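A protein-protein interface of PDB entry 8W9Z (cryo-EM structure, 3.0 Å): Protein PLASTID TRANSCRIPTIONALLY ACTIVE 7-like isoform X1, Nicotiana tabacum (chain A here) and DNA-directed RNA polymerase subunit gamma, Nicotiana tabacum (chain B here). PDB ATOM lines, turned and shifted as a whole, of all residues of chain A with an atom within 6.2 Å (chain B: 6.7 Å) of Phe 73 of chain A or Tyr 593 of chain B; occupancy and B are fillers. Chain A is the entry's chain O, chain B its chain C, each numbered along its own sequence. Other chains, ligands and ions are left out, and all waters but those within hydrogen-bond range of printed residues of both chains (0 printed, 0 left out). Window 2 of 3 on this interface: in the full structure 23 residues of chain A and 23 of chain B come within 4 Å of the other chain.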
ATOM      1  N   ARG A  70     -13.126 -36.990  26.188  1.00  0.00           N
ATOM      2  CA  ARG A  70     -14.486 -36.702  25.745  1.00  0.00           C
ATOM      3  C   ARG A  70     -14.888 -35.279  26.118  1.00  0.00           C
ATOM      4  O   ARG A  70     -15.476 -35.047  27.174  1.00  0.00           O
ATOM      5  CB  ARG A  70     -15.471 -37.706  26.349  1.00  0.00           C
ATOM      6  CG  ARG A  70     -16.888 -37.595  25.810  1.00  0.00           C
ATOM      7  CD  ARG A  70     -16.959 -38.008  24.348  1.00  0.00           C
ATOM      8  NE  ARG A  70     -16.586 -39.406  24.159  1.00  0.00           N
ATOM      9  CZ  ARG A  70     -16.600 -40.032  22.986  1.00  0.00           C
ATOM     10  NH1 ARG A  70     -16.970 -39.383  21.890  1.00  0.00           N
ATOM     11  NH2 ARG A  70     -16.245 -41.308  22.908  1.00  0.00           N
ATOM     12  N   ILE A  71     -14.562 -34.331  25.251  1.00  0.00           N
ATOM     13  CA  ILE A  71     -14.920 -32.931  25.493  1.00  0.00           C
ATOM     14  C   ILE A  71     -16.414 -32.756  25.235  1.00  0.00           C
ATOM     15  O   ILE A  71     -16.906 -33.182  24.177  1.00  0.00           O
ATOM     16  CB  ILE A  71     -14.091 -31.999  24.611  1.00  0.00           C
ATOM     17  CG1 ILE A  71     -12.800 -31.580  25.326  1.00  0.00           C
ATOM     18  CG2 ILE A  71     -14.887 -30.757  24.227  1.00  0.00           C
ATOM     19  CD1 ILE A  71     -11.826 -32.707  25.592  1.00  0.00           C
ATOM     20  N   PRO A  72     -17.164 -32.166  26.170  1.00  0.00           N
ATOM     21  CA  PRO A  72     -18.615 -32.039  25.954  1.00  0.00           C
ATOM     22  C   PRO A  72     -18.976 -31.067  24.847  1.00  0.00           C
ATOM     23  O   PRO A  72     -19.878 -31.353  24.049  1.00  0.00           O
ATOM     24  CB  PRO A  72     -19.130 -31.558  27.320  1.00  0.00           C
ATOM     25  CG  PRO A  72     -18.037 -31.891  28.294  1.00  0.00           C
ATOM     26  CD  PRO A  72     -16.765 -31.752  27.524  1.00  0.00           C
ATOM     27  N   PHE A  73     -18.298 -29.922  24.771  1.00  0.00           N
ATOM     28  CA  PHE A  73     -18.647 -28.866  23.822  1.00  0.00           C
ATOM     29  C   PHE A  73     -17.754 -29.006  22.593  1.00  0.00           C
ATOM     30  O   PHE A  73     -16.805 -28.250  22.384  1.00  0.00           O
ATOM     31  CB  PHE A  73     -18.508 -27.498  24.477  1.00  0.00           C
ATOM     32  CG  PHE A  73     -18.839 -27.494  25.941  1.00  0.00           C
ATOM     33  CD1 PHE A  73     -20.156 -27.461  26.367  1.00  0.00           C
ATOM     34  CD2 PHE A  73     -17.834 -27.526  26.892  1.00  0.00           C
ATOM     35  CE1 PHE A  73     -20.462 -27.460  27.713  1.00  0.00           C
ATOM     36  CE2 PHE A  73     -18.135 -27.524  28.238  1.00  0.00           C
ATOM     37  CZ  PHE A  73     -19.450 -27.490  28.648  1.00  0.00           C
ATOM     38  N   LEU A  74     -18.074 -30.000  21.765  1.00  0.00           N
ATOM     39  CA  LEU A  74     -17.302 -30.254  20.560  1.00  0.00           C
ATOM     40  C   LEU A  74     -18.157 -30.607  19.349  1.00  0.00           C
ATOM     41  O   LEU A  74     -17.596 -30.892  18.286  1.00  0.00           O
ATOM     42  CB  LEU A  74     -16.283 -31.379  20.816  1.00  0.00           C
ATOM     43  CG  LEU A  74     -15.012 -31.368  19.968  1.00  0.00           C
ATOM     44  CD1 LEU A  74     -14.361 -30.002  20.044  1.00  0.00           C
ATOM     45  CD2 LEU A  74     -14.051 -32.453  20.423  1.00  0.00           C
ATOM     46  N   GLU A  75     -19.485 -30.585  19.465  1.00  0.00           N
ATOM     47  CA  GLU A  75     -20.334 -30.976  18.346  1.00  0.00           C
ATOM     48  C   GLU A  75     -20.426 -29.887  17.284  1.00  0.00           C
ATOM     49  O   GLU A  75     -20.658 -30.193  16.107  1.00  0.00           O
ATOM     50  CB  GLU A  75     -21.733 -31.332  18.851  1.00  0.00           C
ATOM     51  CG  GLU A  75     -21.751 -32.439  19.893  1.00  0.00           C
ATOM     52  CD  GLU A  75     -23.150 -32.751  20.387  1.00  0.00           C
ATOM     53  OE1 GLU A  75     -24.106 -32.095  19.923  1.00  0.00           O
ATOM     54  OE2 GLU A  75     -23.294 -33.652  21.239  1.00  0.00           O
ATOM     55  N   GLU A  76     -20.241 -28.624  17.674  1.00  0.00           N
ATOM     56  CA  GLU A  76     -20.386 -27.523  16.727  1.00  0.00           C
ATOM     57  C   GLU A  76     -19.333 -27.602  15.628  1.00  0.00           C
ATOM     58  O   GLU A  76     -19.654 -27.505  14.437  1.00  0.00           O
ATOM     59  CB  GLU A  76     -20.305 -26.186  17.466  1.00  0.00           C
ATOM     60  CG  GLU A  76     -20.788 -24.983  16.660  1.00  0.00           C
ATOM     61  CD  GLU A  76     -19.725 -24.422  15.735  1.00  0.00           C
ATOM     62  OE1 GLU A  76     -18.527 -24.677  15.978  1.00  0.00           O
ATOM     63  OE2 GLU A  76     -20.089 -23.725  14.764  1.00  0.00           O
ATOM     64  N   SER B 590     -11.305 -27.535  39.613  1.00  0.00           N
ATOM     65  CA  SER B 590     -11.122 -28.946  39.296  1.00  0.00           C
ATOM     66  C   SER B 590     -10.991 -29.180  37.797  1.00  0.00           C
ATOM     67  O   SER B 590     -10.304 -30.118  37.378  1.00  0.00           O
ATOM     68  CB  SER B 590     -12.285 -29.764  39.861  1.00  0.00           C
ATOM     69  OG  SER B 590     -12.386 -29.600  41.265  1.00  0.00           O
ATOM     70  N   ASN B 591     -11.633 -28.349  36.980  1.00  0.00           N
ATOM     71  CA  ASN B 591     -11.596 -28.494  35.533  1.00  0.00           C
ATOM     72  C   ASN B 591     -11.370 -27.136  34.885  1.00  0.00           C
ATOM     73  O   ASN B 591     -11.713 -26.094  35.451  1.00  0.00           O
ATOM     74  CB  ASN B 591     -12.893 -29.115  34.997  1.00  0.00           C
ATOM     75  CG  ASN B 591     -13.183 -30.474  35.603  1.00  0.00           C
ATOM     76  OD1 ASN B 591     -14.217 -30.673  36.240  1.00  0.00           O
ATOM     77  ND2 ASN B 591     -12.268 -31.416  35.408  1.00  0.00           N
ATOM     78  N   SER B 592     -10.785 -27.159  33.685  1.00  0.00           N
ATOM     79  CA  SER B 592     -10.585 -25.921  32.939  1.00  0.00           C
ATOM     80  C   SER B 592     -11.909 -25.340  32.460  1.00  0.00           C
ATOM     81  O   SER B 592     -12.010 -24.125  32.238  1.00  0.00           O
ATOM     82  CB  SER B 592      -9.651 -26.165  31.755  1.00  0.00           C
ATOM     83  OG  SER B 592     -10.177 -27.155  30.888  1.00  0.00           O
ATOM     84  N   TYR B 593     -12.927 -26.187  32.291  1.00  0.00           N
ATOM     85  CA  TYR B 593     -14.248 -25.695  31.919  1.00  0.00           C
ATOM     86  C   TYR B 593     -14.795 -24.754  32.981  1.00  0.00           C
ATOM     87  O   TYR B 593     -15.373 -23.709  32.659  1.00  0.00           O
ATOM     88  CB  TYR B 593     -15.204 -26.868  31.699  1.00  0.00           C
ATOM     89  CG  TYR B 593     -14.607 -28.013  30.911  1.00  0.00           C
ATOM     90  CD1 TYR B 593     -14.584 -27.989  29.523  1.00  0.00           C
ATOM     91  CD2 TYR B 593     -14.075 -29.122  31.556  1.00  0.00           C
ATOM     92  CE1 TYR B 593     -14.040 -29.033  28.800  1.00  0.00           C
ATOM     93  CE2 TYR B 593     -13.530 -30.172  30.840  1.00  0.00           C
ATOM     94  CZ  TYR B 593     -13.516 -30.122  29.463  1.00  0.00           C
ATOM     95  OH  TYR B 593     -12.975 -31.165  28.747  1.00  0.00           O
ATOM     96  N   ASP B 594     -14.613 -25.102  34.257  1.00  0.00           N
ATOM     97  CA  ASP B 594     -15.061 -24.226  35.336  1.00  0.00           C
ATOM     98  C   ASP B 594     -14.289 -22.914  35.338  1.00  0.00           C
ATOM     99  O   ASP B 594     -14.858 -21.853  35.616  1.00  0.00           O
ATOM    100  CB  ASP B 594     -14.919 -24.937  36.682  1.00  0.00           C
ATOM    101  CG  ASP B 594     -15.721 -26.221  36.750  1.00  0.00           C
ATOM    102  OD1 ASP B 594     -16.770 -26.306  36.076  1.00  0.00           O
ATOM    103  OD2 ASP B 594     -15.304 -27.146  37.478  1.00  0.00           O
ATOM    104  N   ALA B 595     -12.994 -22.963  35.018  1.00  0.00           N
ATOM    105  CA  ALA B 595     -12.202 -21.738  34.957  1.00  0.00           C
ATOM    106  C   ALA B 595     -12.692 -20.821  33.843  1.00  0.00           C
ATOM    107  O   ALA B 595     -12.844 -19.610  34.045  1.00  0.00           O
ATOM    108  CB  ALA B 595     -10.725 -22.076  34.762  1.00  0.00           C
ATOM    109  N   ILE B 596     -12.950 -21.381  32.659  1.00  0.00           N
ATOM    110  CA  ILE B 596     -13.439 -20.564  31.553  1.00  0.00           C
ATOM    111  C   ILE B 596     -14.838 -20.036  31.854  1.00  0.00           C
ATOM    112  O   ILE B 596     -15.179 -18.904  31.492  1.00  0.00           O
ATOM    113  CB  ILE B 596     -13.394 -21.362  30.238  1.00  0.00           C
ATOM    114  CG1 ILE B 596     -11.947 -21.724  29.895  1.00  0.00           C
ATOM    115  CG2 ILE B 596     -14.024 -20.572  29.102  1.00  0.00           C
ATOM    116  CD1 ILE B 596     -11.773 -22.344  28.528  1.00  0.00           C
ATOM    117  N   GLY B 597     -15.660 -20.832  32.540  1.00  0.00           N
ATOM    118  CA  GLY B 597     -16.981 -20.358  32.917  1.00  0.00           C
ATOM    119  C   GLY B 597     -16.929 -19.226  33.925  1.00  0.00           C
ATOM    120  O   GLY B 597     -17.722 -18.282  33.854  1.00  0.00           O
ATOM    121  N   ALA B 598     -15.998 -19.303  34.878  1.00  0.00           N
ATOM    122  CA  ALA B 598     -15.826 -18.213  35.831  1.00  0.00           C
ATOM    123  C   ALA B 598     -15.259 -16.971  35.159  1.00  0.00           C
ATOM    124  O   ALA B 598     -15.585 -15.848  35.560  1.00  0.00           O
ATOM    125  CB  ALA B 598     -14.922 -18.656  36.981  1.00  0.00           C
ATOM    126  N   ARG B 600     -15.878 -16.129  31.970  1.00  0.00           N
ATOM    127  CA  ARG B 600     -16.979 -15.559  31.202  1.00  0.00           C
ATOM    128  C   ARG B 600     -18.002 -14.881  32.104  1.00  0.00           C
ATOM    129  O   ARG B 600     -18.644 -13.909  31.690  1.00  0.00           O
ATOM    130  CB  ARG B 600     -17.650 -16.640  30.355  1.00  0.00           C
ATOM    131  CG  ARG B 600     -16.769 -17.195  29.247  1.00  0.00           C
ATOM    132  CD  ARG B 600     -17.490 -18.257  28.427  1.00  0.00           C
ATOM    133  NE  ARG B 600     -17.798 -19.452  29.208  1.00  0.00           N
ATOM    134  CZ  ARG B 600     -18.995 -19.724  29.722  1.00  0.00           C
ATOM    135  NH1 ARG B 600     -20.004 -18.884  29.538  1.00  0.00           N
ATOM    136  NH2 ARG B 600     -19.182 -20.836  30.418  1.00  0.00           N
ATOM    137  N   LEU B 612      -5.199 -24.983  38.999  1.00  0.00           N
ATOM    138  CA  LEU B 612      -5.948 -25.942  38.200  1.00  0.00           C
ATOM    139  C   LEU B 612      -5.484 -27.348  38.554  1.00  0.00           C
ATOM    140  O   LEU B 612      -4.296 -27.663  38.433  1.00  0.00           O
ATOM    141  CB  LEU B 612      -5.760 -25.677  36.706  1.00  0.00           C
ATOM    142  CG  LEU B 612      -6.559 -26.580  35.767  1.00  0.00           C
ATOM    143  CD1 LEU B 612      -8.052 -26.350  35.942  1.00  0.00           C
ATOM    144  CD2 LEU B 612      -6.145 -26.360  34.323  1.00  0.00           C
ATOM    145  N   ILE B 667      -4.535 -22.190  29.577  1.00  0.00           N
ATOM    146  CA  ILE B 667      -5.462 -23.315  29.578  1.00  0.00           C
ATOM    147  C   ILE B 667      -6.464 -23.187  28.441  1.00  0.00           C
ATOM    148  O   ILE B 667      -6.884 -24.195  27.868  1.00  0.00           O
ATOM    149  CB  ILE B 667      -6.160 -23.448  30.945  1.00  0.00           C
ATOM    150  CG1 ILE B 667      -6.996 -22.206  31.255  1.00  0.00           C
ATOM    151  CG2 ILE B 667      -5.135 -23.682  32.040  1.00  0.00           C
ATOM    152  CD1 ILE B 667      -7.705 -22.270  32.589  1.00  0.00           C
ATOM    153  N   ARG B 671      -6.750 -26.085  25.725  1.00  0.00           N
ATOM    154  CA  ARG B 671      -8.045 -26.721  25.535  1.00  0.00           C
ATOM    155  C   ARG B 671      -8.514 -26.601  24.094  1.00  0.00           C
ATOM    156  O   ARG B 671      -9.057 -27.559  23.534  1.00  0.00           O
ATOM    157  CB  ARG B 671      -9.076 -26.110  26.486  1.00  0.00           C
ATOM    158  CG  ARG B 671     -10.511 -26.504  26.175  1.00  0.00           C
ATOM    159  CD  ARG B 671     -11.496 -25.831  27.114  1.00  0.00           C
ATOM    160  NE  ARG B 671     -12.872 -25.978  26.645  1.00  0.00           N
ATOM    161  CZ  ARG B 671     -13.940 -25.548  27.308  1.00  0.00           C
ATOM    162  NH1 ARG B 671     -13.799 -24.947  28.481  1.00  0.00           N
ATOM    163  NH2 ARG B 671     -15.151 -25.726  26.800  1.00  0.00           N
ATOM    164  N   GLU B 675      -9.132 -29.810  21.775  1.00  0.00           N
ATOM    165  CA  GLU B 675     -10.476 -30.058  21.275  1.00  0.00           C
ATOM    166  C   GLU B 675     -10.521 -30.018  19.754  1.00  0.00           C
ATOM    167  O   GLU B 675     -11.300 -30.757  19.148  1.00  0.00           O
ATOM    168  CB  GLU B 675     -11.464 -29.057  21.879  1.00  0.00           C
ATOM    169  N   ARG B 682     -12.595 -37.269  15.491  1.00  0.00           N
ATOM    170  CA  ARG B 682     -13.942 -37.828  15.537  1.00  0.00           C
ATOM    171  C   ARG B 682     -14.678 -37.640  14.215  1.00  0.00           C
ATOM    172  O   ARG B 682     -15.358 -38.560  13.747  1.00  0.00           O
ATOM    173  CB  ARG B 682     -14.736 -37.204  16.685  1.00  0.00           C
ATOM    174  CG  ARG B 682     -16.161 -37.718  16.793  1.00  0.00           C
ATOM    175  CD  ARG B 682     -16.713 -37.558  18.199  1.00  0.00           C
ATOM    176  NE  ARG B 682     -16.721 -36.167  18.637  1.00  0.00           N
ATOM    177  CZ  ARG B 682     -17.171 -35.761  19.820  1.00  0.00           C
ATOM    178  NH1 ARG B 682     -17.650 -36.643  20.687  1.00  0.00           N
ATOM    179  NH2 ARG B 682     -17.141 -34.475  20.139  1.00  0.00           N
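Printed residues of chain B within 4 Å of Arg 70 of chain A: Arg 682 (3.1 Å). Of the printed residues of chain B, Ile 71 of chain A touches Tyr 593. Phe 73 of chain A touches just these residues of chain B: Tyr 593 and Arg 671. Of the printed residues of chain B, Leu 74 of chain A touches Glu 675 and Arg 682. Tyr 593 of chain B touches just these residues of chain A: Ile 71 and Phe 73. Printed residues of chain A within 4 Å of Glu 675 of chain B: Leu 74 (3.3 Å). The nearest residue of chain B that does not touch Phe 73 of chain A is Glu 675 of chain B (5.4 Å). The nearest printed residue of chain B that does not touch Arg 70 of chain A is Tyr 593 of chain B (4.9 Å).
Hydrophobic or aromatic side chains of chain B within 4 Å of the printed part of chain A: Tyr 593. Among the printed residues, 6 pairs touch across the chains.
Among the printed residues, pairs that only touch across the chains: Ile 71 of chain A with Tyr 593 of chain B, Phe 73 of chain A with Tyr 593 of chain B, Phe 73 of chain A with Arg 671 of chain B, Leu 74 of chain A with Glu 675 of chain B and Leu 74 of chain A with Arg 682 of chain B.
The guanidinium group (NH1) of Arg 682 of chain B sits close to the guanidinium group (NH1) of Arg 70 of chain A (3.1 Å).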
